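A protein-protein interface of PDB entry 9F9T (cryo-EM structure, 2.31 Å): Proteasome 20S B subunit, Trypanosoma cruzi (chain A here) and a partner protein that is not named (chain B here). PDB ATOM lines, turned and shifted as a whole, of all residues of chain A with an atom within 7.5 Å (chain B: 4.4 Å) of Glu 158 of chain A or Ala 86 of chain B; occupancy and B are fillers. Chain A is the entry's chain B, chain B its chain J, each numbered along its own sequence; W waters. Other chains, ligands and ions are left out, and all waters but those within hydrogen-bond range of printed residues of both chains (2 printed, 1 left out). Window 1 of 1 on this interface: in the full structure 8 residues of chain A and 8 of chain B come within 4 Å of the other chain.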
ATOM      1  N   ASP A 124     -15.170  -5.661  10.040  1.00  0.00           N
ATOM      2  CA  ASP A 124     -13.820  -5.410  10.478  1.00  0.00           C
ATOM      3  C   ASP A 124     -13.582  -6.374  11.616  1.00  0.00           C
ATOM      4  O   ASP A 124     -14.461  -7.143  11.980  1.00  0.00           O
ATOM      5  CB  ASP A 124     -13.602  -3.946  10.852  1.00  0.00           C
ATOM      6  CG  ASP A 124     -12.119  -3.501  10.973  1.00  0.00           C
ATOM      7  OD1 ASP A 124     -11.206  -4.305  10.523  1.00  0.00           O
ATOM      8  OD2 ASP A 124     -11.844  -2.337  11.509  1.00  0.00           O
ATOM      9  N   HIS A 126     -13.717  -6.178  14.670  1.00  0.00           N
ATOM     10  CA  HIS A 126     -14.508  -6.013  15.876  1.00  0.00           C
ATOM     11  C   HIS A 126     -16.007  -5.940  15.632  1.00  0.00           C
ATOM     12  O   HIS A 126     -16.732  -5.661  16.567  1.00  0.00           O
ATOM     13  CB  HIS A 126     -14.140  -4.716  16.575  1.00  0.00           C
ATOM     14  CG  HIS A 126     -14.329  -3.463  15.818  1.00  0.00           C
ATOM     15  ND1 HIS A 126     -13.805  -3.297  14.548  1.00  0.00           N
ATOM     16  CD2 HIS A 126     -15.038  -2.324  16.117  1.00  0.00           C
ATOM     17  CE1 HIS A 126     -14.162  -2.080  14.107  1.00  0.00           C
ATOM     18  NE2 HIS A 126     -14.857  -1.443  15.074  1.00  0.00           N
ATOM     19  N   CYS A 149     -14.768   1.557   7.845  1.00  0.00           N
ATOM     20  CA  CYS A 149     -13.941   1.075   8.946  1.00  0.00           C
ATOM     21  C   CYS A 149     -12.455   1.204   8.676  1.00  0.00           C
ATOM     22  O   CYS A 149     -11.722   1.624   9.559  1.00  0.00           O
ATOM     23  CB  CYS A 149     -14.148  -0.403   9.192  1.00  0.00           C
ATOM     24  SG  CYS A 149     -15.735  -0.800   9.964  1.00  0.00           S
ATOM     25  N   GLN A 150     -11.987   0.833   7.475  1.00  0.00           N
ATOM     26  CA  GLN A 150     -10.553   0.962   7.218  1.00  0.00           C
ATOM     27  C   GLN A 150     -10.162   2.441   7.213  1.00  0.00           C
ATOM     28  O   GLN A 150      -9.167   2.827   7.815  1.00  0.00           O
ATOM     29  CB  GLN A 150     -10.108   0.264   5.938  1.00  0.00           C
ATOM     30  CG  GLN A 150     -10.322  -1.226   6.001  1.00  0.00           C
ATOM     31  CD  GLN A 150      -9.576  -1.836   7.165  1.00  0.00           C
ATOM     32  OE1 GLN A 150      -8.387  -1.582   7.408  1.00  0.00           O
ATOM     33  NE2 GLN A 150     -10.296  -2.692   7.883  1.00  0.00           N
ATOM     34  N   LYS A 151     -10.992   3.261   6.600  1.00  0.00           N
ATOM     35  CA  LYS A 151     -10.791   4.692   6.610  1.00  0.00           C
ATOM     36  C   LYS A 151     -10.654   5.265   8.019  1.00  0.00           C
ATOM     37  O   LYS A 151      -9.830   6.153   8.237  1.00  0.00           O
ATOM     38  CB  LYS A 151     -11.861   5.412   5.779  1.00  0.00           C
ATOM     39  CG  LYS A 151     -11.778   6.913   5.960  1.00  0.00           C
ATOM     40  CD  LYS A 151     -12.656   7.770   5.054  1.00  0.00           C
ATOM     41  CE  LYS A 151     -12.383   9.257   5.282  1.00  0.00           C
ATOM     42  NZ  LYS A 151     -13.613  10.013   5.626  1.00  0.00           N
ATOM     43  N   TYR A 152     -11.417   4.768   8.973  1.00  0.00           N
ATOM     44  CA  TYR A 152     -11.358   5.303  10.321  1.00  0.00           C
ATOM     45  C   TYR A 152     -10.023   4.916  10.974  1.00  0.00           C
ATOM     46  O   TYR A 152      -9.389   5.687  11.682  1.00  0.00           O
ATOM     47  CB  TYR A 152     -12.627   4.760  11.036  1.00  0.00           C
ATOM     48  CG  TYR A 152     -12.826   5.342  12.432  1.00  0.00           C
ATOM     49  CD1 TYR A 152     -13.697   6.393  12.659  1.00  0.00           C
ATOM     50  CD2 TYR A 152     -12.138   4.841  13.525  1.00  0.00           C
ATOM     51  CE1 TYR A 152     -13.861   6.952  13.914  1.00  0.00           C
ATOM     52  CE2 TYR A 152     -12.240   5.424  14.788  1.00  0.00           C
ATOM     53  CZ  TYR A 152     -13.111   6.501  14.981  1.00  0.00           C
ATOM     54  OH  TYR A 152     -13.281   7.053  16.224  1.00  0.00           O
ATOM     55  N   ARG A 153      -9.599   3.670  10.729  1.00  0.00           N
ATOM     56  CA  ARG A 153      -8.305   3.177  11.173  1.00  0.00           C
ATOM     57  C   ARG A 153      -7.192   4.057  10.648  1.00  0.00           C
ATOM     58  O   ARG A 153      -6.346   4.494  11.421  1.00  0.00           O
ATOM     59  CB  ARG A 153      -8.150   1.722  10.741  1.00  0.00           C
ATOM     60  CG  ARG A 153      -8.490   0.754  11.854  1.00  0.00           C
ATOM     61  CD  ARG A 153      -8.349  -0.646  11.322  1.00  0.00           C
ATOM     62  NE  ARG A 153      -9.137  -1.584  12.117  1.00  0.00           N
ATOM     63  CZ  ARG A 153      -8.904  -1.875  13.392  1.00  0.00           C
ATOM     64  NH1 ARG A 153      -9.771  -2.628  14.055  1.00  0.00           N
ATOM     65  NH2 ARG A 153      -7.847  -1.356  13.996  1.00  0.00           N
ATOM     66  N   LEU A 154      -7.176   4.323   9.345  1.00  0.00           N
ATOM     67  CA  LEU A 154      -6.069   5.106   8.789  1.00  0.00           C
ATOM     68  C   LEU A 154      -5.977   6.438   9.471  1.00  0.00           C
ATOM     69  O   LEU A 154      -4.885   6.941   9.615  1.00  0.00           O
ATOM     70  CB  LEU A 154      -6.255   5.364   7.304  1.00  0.00           C
ATOM     71  CG  LEU A 154      -6.037   4.136   6.438  1.00  0.00           C
ATOM     72  CD1 LEU A 154      -6.574   4.396   5.058  1.00  0.00           C
ATOM     73  CD2 LEU A 154      -4.540   3.808   6.303  1.00  0.00           C
ATOM     74  N   THR A 155      -7.119   7.034   9.768  1.00  0.00           N
ATOM     75  CA  THR A 155      -7.155   8.326  10.401  1.00  0.00           C
ATOM     76  C   THR A 155      -6.829   8.210  11.867  1.00  0.00           C
ATOM     77  O   THR A 155      -6.046   9.036  12.291  1.00  0.00           O
ATOM     78  CB  THR A 155      -8.513   9.014  10.229  1.00  0.00           C
ATOM     79  OG1 THR A 155      -8.778   9.144   8.851  1.00  0.00           O
ATOM     80  CG2 THR A 155      -8.574  10.405  10.779  1.00  0.00           C
ATOM     81  N   TYR A 156      -7.429   7.352  12.683  1.00  0.00           N
ATOM     82  CA  TYR A 156      -7.295   7.495  14.139  1.00  0.00           C
ATOM     83  C   TYR A 156      -6.499   6.356  14.779  1.00  0.00           C
ATOM     84  O   TYR A 156      -6.319   6.348  15.993  1.00  0.00           O
ATOM     85  CB  TYR A 156      -8.666   7.572  14.806  1.00  0.00           C
ATOM     86  CG  TYR A 156      -9.561   8.721  14.337  1.00  0.00           C
ATOM     87  CD1 TYR A 156      -9.399   9.983  14.881  1.00  0.00           C
ATOM     88  CD2 TYR A 156     -10.517   8.557  13.333  1.00  0.00           C
ATOM     89  CE1 TYR A 156     -10.163  11.064  14.456  1.00  0.00           C
ATOM     90  CE2 TYR A 156     -11.326   9.609  12.941  1.00  0.00           C
ATOM     91  CZ  TYR A 156     -11.131  10.888  13.472  1.00  0.00           C
ATOM     92  OH  TYR A 156     -11.806  12.025  13.043  1.00  0.00           O
ATOM     93  N   HIS A 157      -6.105   5.340  13.969  1.00  0.00           N
ATOM     94  CA  HIS A 157      -5.302   4.192  14.401  1.00  0.00           C
ATOM     95  C   HIS A 157      -6.031   3.480  15.520  1.00  0.00           C
ATOM     96  O   HIS A 157      -5.405   3.163  16.541  1.00  0.00           O
ATOM     97  CB  HIS A 157      -3.911   4.534  14.997  1.00  0.00           C
ATOM     98  CG  HIS A 157      -2.950   5.021  13.971  1.00  0.00           C
ATOM     99  ND1 HIS A 157      -1.762   5.682  14.204  1.00  0.00           N
ATOM    100  CD2 HIS A 157      -3.063   4.983  12.601  1.00  0.00           C
ATOM    101  CE1 HIS A 157      -1.216   6.055  13.031  1.00  0.00           C
ATOM    102  NE2 HIS A 157      -1.961   5.620  12.040  1.00  0.00           N
ATOM    103  N   GLU A 158      -7.341   3.335  15.361  1.00  0.00           N
ATOM    104  CA  GLU A 158      -8.105   2.511  16.265  1.00  0.00           C
ATOM    105  C   GLU A 158      -9.391   2.126  15.550  1.00  0.00           C
ATOM    106  O   GLU A 158      -9.737   2.683  14.516  1.00  0.00           O
ATOM    107  CB  GLU A 158      -8.327   3.255  17.588  1.00  0.00           C
ATOM    108  CG  GLU A 158      -9.361   4.337  17.537  1.00  0.00           C
ATOM    109  CD  GLU A 158      -9.804   4.919  18.874  1.00  0.00           C
ATOM    110  OE1 GLU A 158      -8.955   5.149  19.756  1.00  0.00           O
ATOM    111  OE2 GLU A 158     -11.038   5.196  18.999  1.00  0.00           O
ATOM    112  N   PRO A 159     -10.072   1.105  16.075  1.00  0.00           N
ATOM    113  CA  PRO A 159     -11.287   0.563  15.474  1.00  0.00           C
ATOM    114  C   PRO A 159     -12.469   1.524  15.537  1.00  0.00           C
ATOM    115  O   PRO A 159     -12.612   2.203  16.521  1.00  0.00           O
ATOM    116  CB  PRO A 159     -11.598  -0.722  16.286  1.00  0.00           C
ATOM    117  CG  PRO A 159     -10.845  -0.501  17.582  1.00  0.00           C
ATOM    118  CD  PRO A 159      -9.678   0.423  17.305  1.00  0.00           C
ATOM    119  N   MET A 160     -13.200   1.658  14.425  1.00  0.00           N
ATOM    120  CA  MET A 160     -14.294   2.587  14.363  1.00  0.00           C
ATOM    121  C   MET A 160     -15.348   2.129  15.364  1.00  0.00           C
ATOM    122  O   MET A 160     -15.731   0.967  15.315  1.00  0.00           O
ATOM    123  CB  MET A 160     -14.933   2.538  12.974  1.00  0.00           C
ATOM    124  CG  MET A 160     -16.134   3.464  12.788  1.00  0.00           C
ATOM    125  SD  MET A 160     -16.471   3.413  11.063  1.00  0.00           S
ATOM    126  CE  MET A 160     -17.062   5.079  10.772  1.00  0.00           C
ATOM    127  N   PRO A 161     -15.810   2.948  16.313  1.00  0.00           N
ATOM    128  CA  PRO A 161     -16.889   2.536  17.201  1.00  0.00           C
ATOM    129  C   PRO A 161     -18.170   2.163  16.453  1.00  0.00           C
ATOM    130  O   PRO A 161     -18.516   2.802  15.463  1.00  0.00           O
ATOM    131  CB  PRO A 161     -17.189   3.735  18.112  1.00  0.00           C
ATOM    132  CG  PRO A 161     -16.173   4.797  17.765  1.00  0.00           C
ATOM    133  CD  PRO A 161     -15.290   4.274  16.615  1.00  0.00           C
ATOM    134  N   SER A 196     -14.805   0.503  22.854  1.00  0.00           N
ATOM    135  CA  SER A 196     -14.519   0.952  24.218  1.00  0.00           C
ATOM    136  C   SER A 196     -15.787   1.177  25.067  1.00  0.00           C
ATOM    137  O   SER A 196     -15.686   1.257  26.279  1.00  0.00           O
ATOM    138  CB  SER A 196     -13.677   2.208  24.240  1.00  0.00           C
ATOM    139  OG  SER A 196     -12.521   2.087  23.440  1.00  0.00           O
ATOM    140  N   ARG B  80     -17.817  11.758  22.844  1.00  0.00           N
ATOM    141  CA  ARG B  80     -16.762  11.451  23.790  1.00  0.00           C
ATOM    142  C   ARG B  80     -15.532  12.260  23.442  1.00  0.00           C
ATOM    143  O   ARG B  80     -15.471  12.899  22.395  1.00  0.00           O
ATOM    144  CB  ARG B  80     -16.380   9.963  23.776  1.00  0.00           C
ATOM    145  CG  ARG B  80     -15.892   9.484  22.427  1.00  0.00           C
ATOM    146  CD  ARG B  80     -15.148   8.178  22.433  1.00  0.00           C
ATOM    147  NE  ARG B  80     -14.779   7.727  21.092  1.00  0.00           N
ATOM    148  CZ  ARG B  80     -13.993   6.687  20.888  1.00  0.00           C
ATOM    149  NH1 ARG B  80     -13.483   6.098  21.946  1.00  0.00           N
ATOM    150  NH2 ARG B  80     -13.682   6.244  19.673  1.00  0.00           N
ATOM    151  N   ILE B  82     -11.509  12.624  22.711  1.00  0.00           N
ATOM    152  CA  ILE B  82     -10.607  11.841  21.943  1.00  0.00           C
ATOM    153  C   ILE B  82      -9.469  11.444  22.896  1.00  0.00           C
ATOM    154  O   ILE B  82      -9.071  12.247  23.764  1.00  0.00           O
ATOM    155  CB  ILE B  82     -10.251  12.638  20.674  1.00  0.00           C
ATOM    156  CG1 ILE B  82      -9.357  11.830  19.751  1.00  0.00           C
ATOM    157  CG2 ILE B  82      -9.597  13.955  20.945  1.00  0.00           C
ATOM    158  CD1 ILE B  82      -9.238  12.449  18.437  1.00  0.00           C
ATOM    159  N   GLY B  83      -8.916  10.216  22.726  1.00  0.00           N
ATOM    160  CA  GLY B  83      -7.736   9.795  23.492  1.00  0.00           C
ATOM    161  C   GLY B  83      -6.441  10.251  22.812  1.00  0.00           C
ATOM    162  O   GLY B  83      -6.476  10.598  21.629  1.00  0.00           O
ATOM    163  N   GLY B  84      -5.344  10.307  23.609  1.00  0.00           N
ATOM    164  CA  GLY B  84      -4.064  10.882  23.268  1.00  0.00           C
ATOM    165  C   GLY B  84      -3.552  10.265  21.987  1.00  0.00           C
ATOM    166  O   GLY B  84      -2.950  10.939  21.143  1.00  0.00           O
ATOM    167  N   LYS B  85      -3.741   8.945  21.846  1.00  0.00           N
ATOM    168  CA  LYS B  85      -3.207   8.246  20.696  1.00  0.00           C
ATOM    169  C   LYS B  85      -4.016   8.490  19.452  1.00  0.00           C
ATOM    170  O   LYS B  85      -3.490   8.503  18.375  1.00  0.00           O
ATOM    171  CB  LYS B  85      -3.146   6.739  20.920  1.00  0.00           C
ATOM    172  CG  LYS B  85      -1.793   6.196  21.347  1.00  0.00           C
ATOM    173  CD  LYS B  85      -1.880   4.900  22.139  1.00  0.00           C
ATOM    174  CE  LYS B  85      -0.524   4.369  22.565  1.00  0.00           C
ATOM    175  NZ  LYS B  85      -0.631   3.613  23.833  1.00  0.00           N
ATOM    176  N   ALA B  86      -5.305   8.610  19.538  1.00  0.00           N
ATOM    177  CA  ALA B  86      -6.039   8.882  18.329  1.00  0.00           C
ATOM    178  C   ALA B  86      -5.813  10.306  17.875  1.00  0.00           C
ATOM    179  O   ALA B  86      -5.925  10.599  16.689  1.00  0.00           O
ATOM    180  CB  ALA B  86      -7.500   8.585  18.588  1.00  0.00           C
ATOM    181  N   PHE B  87      -5.614  11.215  18.846  1.00  0.00           N
ATOM    182  CA  PHE B  87      -5.438  12.609  18.543  1.00  0.00           C
ATOM    183  C   PHE B  87      -4.140  12.797  17.810  1.00  0.00           C
ATOM    184  O   PHE B  87      -4.077  13.529  16.817  1.00  0.00           O
ATOM    185  CB  PHE B  87      -5.363  13.432  19.788  1.00  0.00           C
ATOM    186  CG  PHE B  87      -5.121  14.900  19.574  1.00  0.00           C
ATOM    187  CD1 PHE B  87      -6.090  15.695  19.016  1.00  0.00           C
ATOM    188  CD2 PHE B  87      -3.918  15.478  19.936  1.00  0.00           C
ATOM    189  CE1 PHE B  87      -5.833  17.042  18.796  1.00  0.00           C
ATOM    190  CE2 PHE B  87      -3.680  16.821  19.746  1.00  0.00           C
ATOM    191  CZ  PHE B  87      -4.653  17.621  19.222  1.00  0.00           C
ATOM    192  N   ALA B  88      -3.135  12.055  18.224  1.00  0.00           N
ATOM    193  CA  ALA B  88      -1.867  12.081  17.534  1.00  0.00           C
ATOM    194  C   ALA B  88      -1.909  11.466  16.164  1.00  0.00           C
ATOM    195  O   ALA B  88      -1.149  11.896  15.303  1.00  0.00           O
ATOM    196  CB  ALA B  88      -0.829  11.331  18.327  1.00  0.00           C
ATOM    197  N   ALA B  89      -2.586  10.343  16.017  1.00  0.00           N
ATOM    198  CA  ALA B  89      -2.725   9.798  14.687  1.00  0.00           C
ATOM    199  C   ALA B  89      -3.468  10.810  13.815  1.00  0.00           C
ATOM    200  O   ALA B  89      -3.305  10.820  12.607  1.00  0.00           O
ATOM    201  CB  ALA B  89      -3.517   8.490  14.696  1.00  0.00           C
ATOM    202  N   LEU B  90      -4.398  11.570  14.403  1.00  0.00           N
ATOM    203  CA  LEU B  90      -5.186  12.484  13.589  1.00  0.00           C
ATOM    204  C   LEU B  90      -4.305  13.624  13.107  1.00  0.00           C
ATOM    205  O   LEU B  90      -4.374  13.956  11.940  1.00  0.00           O
ATOM    206  CB  LEU B  90      -6.347  13.030  14.414  1.00  0.00           C
ATOM    207  CG  LEU B  90      -7.016  14.279  13.823  1.00  0.00           C
ATOM    208  CD1 LEU B  90      -7.945  13.922  12.697  1.00  0.00           C
ATOM    209  CD2 LEU B  90      -7.743  15.106  14.894  1.00  0.00           C
HETATM  210  O   HOH W   1     -15.214   3.145  21.384  1.00  0.00           O
HETATM  211  O   HOH W   2      -7.361   7.146  21.856  1.00  0.00           O
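The guanidinium group (NH2) of Arg 80 of chain B is in salt-bridge range of the side-chain carboxylate (OE2) of Glu 158 of chain A. The backbone carbonyl oxygen (O) of Thr 155 of chain A sits close to the backbone carbonyl oxygen (O) of Ala 89 of chain B (3.3 Å).
Among the printed residues, pairs that only touch across the chains: Tyr 152 of chain A with Arg 80 of chain B (3.6 Å), Thr 155 of chain A with Leu 90 of chain B (3.7 Å), Tyr 156 of chain A with Ala 86 of chain B (3.5 Å), Tyr 156 of chain A with Ala 89 of chain B (3.7 Å), His 157 of chain A with Ala 89 of chain B (3.3 Å), Glu 158 of chain A with Ala 86 of chain B (3.9 Å) and Pro 161 of chain A with Arg 80 of chain B (3.5 Å).
O of Lys 151 of chain A lies within hydrogen-bond range of OG1 of Thr 155 of chain A (3.2 Å).
Of the 16 printed residues of chain A, 6 touch a printed residue of chain B. Hydrophobic or aromatic side chains of chain A that line the printed part of chain B: Tyr 152, Tyr 156, His 157 and Pro 161. Hydrophobic or aromatic side chains of chain B within 4 Å of the printed part of chain A: Ala 86 and Ala 89. Along chain B the printed residues that touch a printed residue of chain A span positions 80 to 90. Among the printed residues, 9 pairs touch across the chains. Among the printed residues, Asp or Glu carboxylates within 4 Å of a Lys or Arg side-chain nitrogen of the other chain: Glu 158 of chain A with Arg 80 of chain B.
Ala 86 of chain B touches two residues of chain A. Of the printed residues of chain A, Leu 90 of chain B touches Thr 155 (3.7 Å). Printed residues of chain B within 4 Å of Tyr 152 of chain A: Arg 80. Of the printed residues of chain A, Ala 89 of chain B touches Thr 155, Tyr 156 and His 157. Lys 151 of chain A touches none of the printed residues of chain B. Ala 88 of chain B touches none of the printed residues of chain A. The nearest printed residue of chain B that does not touch Glu 158 of chain A is Gly 83 of chain B (5.9 Å). The nearest residue of chain A that does not touch Ala 86 of chain B is Thr 155 of chain A (4.7 Å).
Water W1 lies within hydrogen-bond range of the backbone NH of Ser 196 of chain A (3.1 Å) and the guanidinium group of Arg 80 of chain B (3.5 Å). Water W2 lies within hydrogen-bond range of the side-chain carboxylate (OE1) of Glu 158 of chain A (3.3 Å) and the backbone NH (N) of Ala 86 of chain B (3.4 Å).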
